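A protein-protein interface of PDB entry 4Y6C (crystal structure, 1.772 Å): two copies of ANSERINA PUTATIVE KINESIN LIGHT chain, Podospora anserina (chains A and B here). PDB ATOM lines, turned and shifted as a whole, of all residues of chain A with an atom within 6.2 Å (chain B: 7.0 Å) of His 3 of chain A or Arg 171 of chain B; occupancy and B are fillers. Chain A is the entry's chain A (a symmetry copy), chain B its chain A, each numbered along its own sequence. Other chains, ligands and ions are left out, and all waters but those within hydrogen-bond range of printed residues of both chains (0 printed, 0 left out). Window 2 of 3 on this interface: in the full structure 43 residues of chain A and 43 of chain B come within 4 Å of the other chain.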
ATOM      1  N   HIS A   3      18.571 -22.718  -0.594  1.00  0.00           N
ATOM      2  CA  HIS A   3      19.803 -22.188  -1.160  1.00  0.00           C
ATOM      3  C   HIS A   3      19.782 -20.655  -1.155  1.00  0.00           C
ATOM      4  O   HIS A   3      20.831 -20.016  -1.197  1.00  0.00           O
ATOM      5  CB  HIS A   3      20.016 -22.734  -2.580  1.00  0.00           C
ATOM      6  CG  HIS A   3      21.193 -22.140  -3.291  1.00  0.00           C
ATOM      7  ND1 HIS A   3      21.133 -21.712  -4.601  1.00  0.00           N
ATOM      8  CD2 HIS A   3      22.460 -21.906  -2.878  1.00  0.00           C
ATOM      9  CE1 HIS A   3      22.312 -21.238  -4.961  1.00  0.00           C
ATOM     10  NE2 HIS A   3      23.135 -21.342  -3.933  1.00  0.00           N
ATOM     11  N   MET A   4      18.585 -20.072  -1.116  1.00  0.00           N
ATOM     12  CA  MET A   4      18.411 -18.629  -0.956  1.00  0.00           C
ATOM     13  C   MET A   4      19.155 -18.183   0.304  1.00  0.00           C
ATOM     14  O   MET A   4      19.108 -18.881   1.315  1.00  0.00           O
ATOM     15  CB  MET A   4      16.912 -18.299  -0.888  1.00  0.00           C
ATOM     16  CG  MET A   4      16.524 -16.972  -0.284  1.00  0.00           C
ATOM     17  SD  MET A   4      14.560 -16.939  -0.034  1.00  0.00           S
ATOM     18  CE  MET A   4      14.035 -17.483  -1.853  1.00  0.00           C
ATOM     19  N   GLU A   5      19.830 -17.036   0.247  1.00  0.00           N
ATOM     20  CA  GLU A   5      20.729 -16.602   1.326  1.00  0.00           C
ATOM     21  C   GLU A   5      20.082 -16.412   2.696  1.00  0.00           C
ATOM     22  O   GLU A   5      20.623 -16.862   3.710  1.00  0.00           O
ATOM     23  CB  GLU A   5      21.423 -15.299   0.927  1.00  0.00           C
ATOM     24  CG  GLU A   5      22.443 -14.784   1.948  1.00  0.00           C
ATOM     25  CD  GLU A   5      23.818 -15.415   1.787  1.00  0.00           C
ATOM     26  OE1 GLU A   5      23.962 -16.349   0.967  1.00  0.00           O
ATOM     27  OE2 GLU A   5      24.758 -14.971   2.481  1.00  0.00           O
ATOM     28  N   HIS A   6      18.938 -15.734   2.732  1.00  0.00           N
ATOM     29  CA  HIS A   6      18.314 -15.384   4.002  1.00  0.00           C
ATOM     30  C   HIS A   6      16.850 -15.785   4.040  1.00  0.00           C
ATOM     31  O   HIS A   6      15.981 -14.926   4.011  1.00  0.00           O
ATOM     32  CB  HIS A   6      18.433 -13.879   4.254  1.00  0.00           C
ATOM     33  CG  HIS A   6      19.842 -13.392   4.392  1.00  0.00           C
ATOM     34  ND1 HIS A   6      20.703 -13.866   5.362  1.00  0.00           N
ATOM     35  CD2 HIS A   6      20.537 -12.463   3.693  1.00  0.00           C
ATOM     36  CE1 HIS A   6      21.869 -13.256   5.246  1.00  0.00           C
ATOM     37  NE2 HIS A   6      21.794 -12.399   4.242  1.00  0.00           N
ATOM     38  N   ILE A  39      10.123 -23.344   1.265  1.00  0.00           N
ATOM     39  CA  ILE A  39      11.507 -22.873   1.178  1.00  0.00           C
ATOM     40  C   ILE A  39      12.178 -22.927   2.551  1.00  0.00           C
ATOM     41  O   ILE A  39      13.312 -23.399   2.697  1.00  0.00           O
ATOM     42  CB  ILE A  39      11.571 -21.438   0.632  1.00  0.00           C
ATOM     43  CG1 ILE A  39      11.131 -21.420  -0.831  1.00  0.00           C
ATOM     44  CG2 ILE A  39      12.975 -20.875   0.785  1.00  0.00           C
ATOM     45  CD1 ILE A  39      10.940 -20.002  -1.413  1.00  0.00           C
ATOM     46  N   LYS A  42      13.434 -26.286   4.057  1.00  0.00           N
ATOM     47  CA  LYS A  42      14.663 -26.868   3.524  1.00  0.00           C
ATOM     48  C   LYS A  42      15.899 -26.281   4.172  1.00  0.00           C
ATOM     49  O   LYS A  42      16.998 -26.802   3.992  1.00  0.00           O
ATOM     50  CB  LYS A  42      14.752 -26.656   2.010  1.00  0.00           C
ATOM     51  CG  LYS A  42      13.654 -27.358   1.217  1.00  0.00           C
ATOM     52  CD  LYS A  42      13.918 -27.207  -0.282  1.00  0.00           C
ATOM     53  CE  LYS A  42      12.667 -27.491  -1.093  1.00  0.00           C
ATOM     54  NZ  LYS A  42      12.157 -28.861  -0.822  1.00  0.00           N
ATOM     55  N   THR A  43      15.720 -25.193   4.920  1.00  0.00           N
ATOM     56  CA  THR A  43      16.851 -24.376   5.327  1.00  0.00           C
ATOM     57  C   THR A  43      16.883 -24.062   6.830  1.00  0.00           C
ATOM     58  O   THR A  43      17.962 -23.877   7.396  1.00  0.00           O
ATOM     59  CB  THR A  43      16.866 -23.051   4.525  1.00  0.00           C
ATOM     60  OG1 THR A  43      15.582 -22.416   4.627  1.00  0.00           O
ATOM     61  CG2 THR A  43      17.131 -23.333   3.057  1.00  0.00           C
ATOM     62  N   GLN B 166      11.909  -8.568 -11.757  1.00  0.00           N
ATOM     63  CA  GLN B 166      12.111  -9.667 -10.814  1.00  0.00           C
ATOM     64  C   GLN B 166      13.043 -10.733 -11.372  1.00  0.00           C
ATOM     65  O   GLN B 166      13.755 -11.402 -10.624  1.00  0.00           O
ATOM     66  CB  GLN B 166      10.769 -10.285 -10.436  1.00  0.00           C
ATOM     67  CG  GLN B 166       9.928  -9.374  -9.558  1.00  0.00           C
ATOM     68  CD  GLN B 166       8.517  -9.890  -9.410  1.00  0.00           C
ATOM     69  OE1 GLN B 166       8.033 -10.647 -10.257  1.00  0.00           O
ATOM     70  NE2 GLN B 166       7.850  -9.494  -8.336  1.00  0.00           N
ATOM     71  N   ALA B 167      13.044 -10.889 -12.691  1.00  0.00           N
ATOM     72  CA  ALA B 167      13.909 -11.869 -13.322  1.00  0.00           C
ATOM     73  C   ALA B 167      15.374 -11.528 -13.059  1.00  0.00           C
ATOM     74  O   ALA B 167      16.237 -12.399 -13.094  1.00  0.00           O
ATOM     75  CB  ALA B 167      13.634 -11.942 -14.804  1.00  0.00           C
ATOM     76  N   LYS B 168      15.642 -10.258 -12.774  1.00  0.00           N
ATOM     77  CA  LYS B 168      17.004  -9.788 -12.535  1.00  0.00           C
ATOM     78  C   LYS B 168      17.338  -9.641 -11.055  1.00  0.00           C
ATOM     79  O   LYS B 168      18.480  -9.356 -10.708  1.00  0.00           O
ATOM     80  CB  LYS B 168      17.230  -8.433 -13.218  1.00  0.00           C
ATOM     81  CG  LYS B 168      16.885  -8.376 -14.698  1.00  0.00           C
ATOM     82  CD  LYS B 168      16.696  -6.924 -15.134  1.00  0.00           C
ATOM     83  CE  LYS B 168      17.526  -6.584 -16.364  1.00  0.00           C
ATOM     84  NZ  LYS B 168      18.240  -5.283 -16.200  1.00  0.00           N
ATOM     85  N   THR B 169      16.346  -9.811 -10.184  1.00  0.00           N
ATOM     86  CA  THR B 169      16.521  -9.459  -8.773  1.00  0.00           C
ATOM     87  C   THR B 169      16.183 -10.588  -7.797  1.00  0.00           C
ATOM     88  O   THR B 169      16.725 -10.638  -6.686  1.00  0.00           O
ATOM     89  CB  THR B 169      15.660  -8.237  -8.393  1.00  0.00           C
ATOM     90  OG1 THR B 169      14.273  -8.549  -8.574  1.00  0.00           O
ATOM     91  CG2 THR B 169      16.019  -7.029  -9.250  1.00  0.00           C
ATOM     92  N   LEU B 170      15.285 -11.477  -8.208  1.00  0.00           N
ATOM     93  CA  LEU B 170      14.794 -12.550  -7.343  1.00  0.00           C
ATOM     94  C   LEU B 170      15.084 -13.928  -7.939  1.00  0.00           C
ATOM     95  O   LEU B 170      15.123 -14.081  -9.153  1.00  0.00           O
ATOM     96  CB  LEU B 170      13.285 -12.395  -7.114  1.00  0.00           C
ATOM     97  CG  LEU B 170      12.767 -11.101  -6.491  1.00  0.00           C
ATOM     98  CD1 LEU B 170      11.233 -11.112  -6.409  1.00  0.00           C
ATOM     99  CD2 LEU B 170      13.390 -10.864  -5.117  1.00  0.00           C
ATOM    100  N   ARG B 171      15.281 -14.937  -7.085  1.00  0.00           N
ATOM    101  CA  ARG B 171      15.459 -16.311  -7.559  1.00  0.00           C
ATOM    102  C   ARG B 171      14.143 -16.865  -8.103  1.00  0.00           C
ATOM    103  O   ARG B 171      13.078 -16.401  -7.705  1.00  0.00           O
ATOM    104  CB  ARG B 171      15.977 -17.196  -6.425  1.00  0.00           C
ATOM    105  CG  ARG B 171      17.376 -16.829  -5.960  1.00  0.00           C
ATOM    106  CD  ARG B 171      17.659 -17.394  -4.577  1.00  0.00           C
ATOM    107  NE  ARG B 171      17.439 -18.837  -4.527  1.00  0.00           N
ATOM    108  CZ  ARG B 171      18.400 -19.737  -4.677  1.00  0.00           C
ATOM    109  NH1 ARG B 171      19.644 -19.336  -4.895  1.00  0.00           N
ATOM    110  NH2 ARG B 171      18.116 -21.031  -4.621  1.00  0.00           N
ATOM    111  N   SER B 172      14.210 -17.859  -8.991  1.00  0.00           N
ATOM    112  CA  SER B 172      13.001 -18.321  -9.667  1.00  0.00           C
ATOM    113  C   SER B 172      11.965 -18.869  -8.676  1.00  0.00           C
ATOM    114  O   SER B 172      10.765 -18.833  -8.946  1.00  0.00           O
ATOM    115  CB  SER B 172      13.340 -19.373 -10.719  1.00  0.00           C
ATOM    116  OG  SER B 172      13.768 -20.573 -10.118  1.00  0.00           O
ATOM    117  N   GLU B 173      12.429 -19.344  -7.522  1.00  0.00           N
ATOM    118  CA  GLU B 173      11.539 -19.980  -6.548  1.00  0.00           C
ATOM    119  C   GLU B 173      10.906 -18.972  -5.588  1.00  0.00           C
ATOM    120  O   GLU B 173      10.016 -19.326  -4.822  1.00  0.00           O
ATOM    121  CB  GLU B 173      12.302 -21.050  -5.752  1.00  0.00           C
ATOM    122  CG  GLU B 173      13.277 -20.455  -4.739  1.00  0.00           C
ATOM    123  CD  GLU B 173      14.173 -21.488  -4.082  1.00  0.00           C
ATOM    124  OE1 GLU B 173      13.937 -22.699  -4.281  1.00  0.00           O
ATOM    125  OE2 GLU B 173      15.114 -21.086  -3.362  1.00  0.00           O
ATOM    126  N   HIS B 174      11.351 -17.715  -5.637  1.00  0.00           N
ATOM    127  CA  HIS B 174      10.851 -16.695  -4.712  1.00  0.00           C
ATOM    128  C   HIS B 174       9.334 -16.517  -4.821  1.00  0.00           C
ATOM    129  O   HIS B 174       8.809 -16.328  -5.917  1.00  0.00           O
ATOM    130  CB  HIS B 174      11.545 -15.353  -4.964  1.00  0.00           C
ATOM    131  CG  HIS B 174      11.268 -14.337  -3.901  1.00  0.00           C
ATOM    132  ND1 HIS B 174      12.230 -13.897  -3.016  1.00  0.00           N
ATOM    133  CD2 HIS B 174      10.127 -13.696  -3.563  1.00  0.00           C
ATOM    134  CE1 HIS B 174      11.693 -13.021  -2.184  1.00  0.00           C
ATOM    135  NE2 HIS B 174      10.421 -12.874  -2.501  1.00  0.00           N
ATOM    136  N   PRO B 175       8.619 -16.583  -3.685  1.00  0.00           N
ATOM    137  CA  PRO B 175       7.150 -16.473  -3.707  1.00  0.00           C
ATOM    138  C   PRO B 175       6.625 -15.244  -4.458  1.00  0.00           C
ATOM    139  O   PRO B 175       5.604 -15.337  -5.135  1.00  0.00           O
ATOM    140  CB  PRO B 175       6.786 -16.386  -2.221  1.00  0.00           C
ATOM    141  CG  PRO B 175       7.875 -17.143  -1.537  1.00  0.00           C
ATOM    142  CD  PRO B 175       9.135 -16.906  -2.339  1.00  0.00           C
ATOM    143  N   ARG B 177       8.107 -13.636  -6.946  1.00  0.00           N
ATOM    144  CA  ARG B 177       8.354 -13.782  -8.382  1.00  0.00           C
ATOM    145  C   ARG B 177       7.269 -14.659  -8.993  1.00  0.00           C
ATOM    146  O   ARG B 177       6.718 -14.347 -10.044  1.00  0.00           O
ATOM    147  CB  ARG B 177       9.750 -14.357  -8.644  1.00  0.00           C
ATOM    148  CG  ARG B 177      10.166 -14.260 -10.098  1.00  0.00           C
ATOM    149  CD  ARG B 177      11.644 -14.539 -10.307  1.00  0.00           C
ATOM    150  NE  ARG B 177      11.900 -14.805 -11.721  1.00  0.00           N
ATOM    151  CZ  ARG B 177      13.054 -15.243 -12.208  1.00  0.00           C
ATOM    152  NH1 ARG B 177      14.086 -15.458 -11.400  1.00  0.00           N
ATOM    153  NH2 ARG B 177      13.176 -15.461 -13.509  1.00  0.00           N
ATOM    154  N   LEU B 178       6.932 -15.744  -8.309  1.00  0.00           N
ATOM    155  CA  LEU B 178       5.851 -16.618  -8.770  1.00  0.00           C
ATOM    156  C   LEU B 178       4.499 -15.902  -8.757  1.00  0.00           C
ATOM    157  O   LEU B 178       3.692 -16.069  -9.671  1.00  0.00           O
ATOM    158  CB  LEU B 178       5.789 -17.873  -7.901  1.00  0.00           C
ATOM    159  CG  LEU B 178       7.058 -18.716  -8.014  1.00  0.00           C
ATOM    160  CD1 LEU B 178       7.056 -19.774  -6.925  1.00  0.00           C
ATOM    161  CD2 LEU B 178       7.130 -19.361  -9.385  1.00  0.00           C
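The guanidinium group (NH1) of Arg 171 of chain B is in hydrogen-bond range of a ring nitrogen (ND1) of His 3 of chain A.
The side-chain carboxylate of Glu 173 of chain B is in salt-bridge range of the guanidinium group of Arg 171 of chain B (3.3 Å).
The backbone carbonyl oxygen (O) of Ile 39 of chain A is in hydrogen-bond range of the side-chain hydroxyl (OG1) of Thr 43 of chain A (3.1 Å).
Among the printed residues, pairs that only touch across the chains: Met 4 of chain A with Arg 171 of chain B (3.6 Å), Ile 39 of chain A with Glu 173 of chain B (3.6 Å) and Ile 39 of chain A with Pro 175 of chain B (3.7 Å).
Of the printed residues of chain A, Arg 171 of chain B touches His 3 and Met 4.
Printed residues of chain B within 4 Å of Met 4 of chain A: Arg 171.
Printed residues of chain A within 4 Å of Pro 175 of chain B: Ile 39.
Printed residues of chain B within 4 Å of Ile 39 of chain A: Glu 173 and Pro 175.
Ala 167 of chain B touches none of the printed residues of chain A.
His 6 of chain A touches none of the printed residues of chain B.
Hydrophobic or aromatic side chains of chain B that line the printed part of chain A: Pro 175.
No position is printed for both chains.
Of the 4 pairs that touch across the chains among the printed residues, none has its exchanged pair printed and touching as well.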
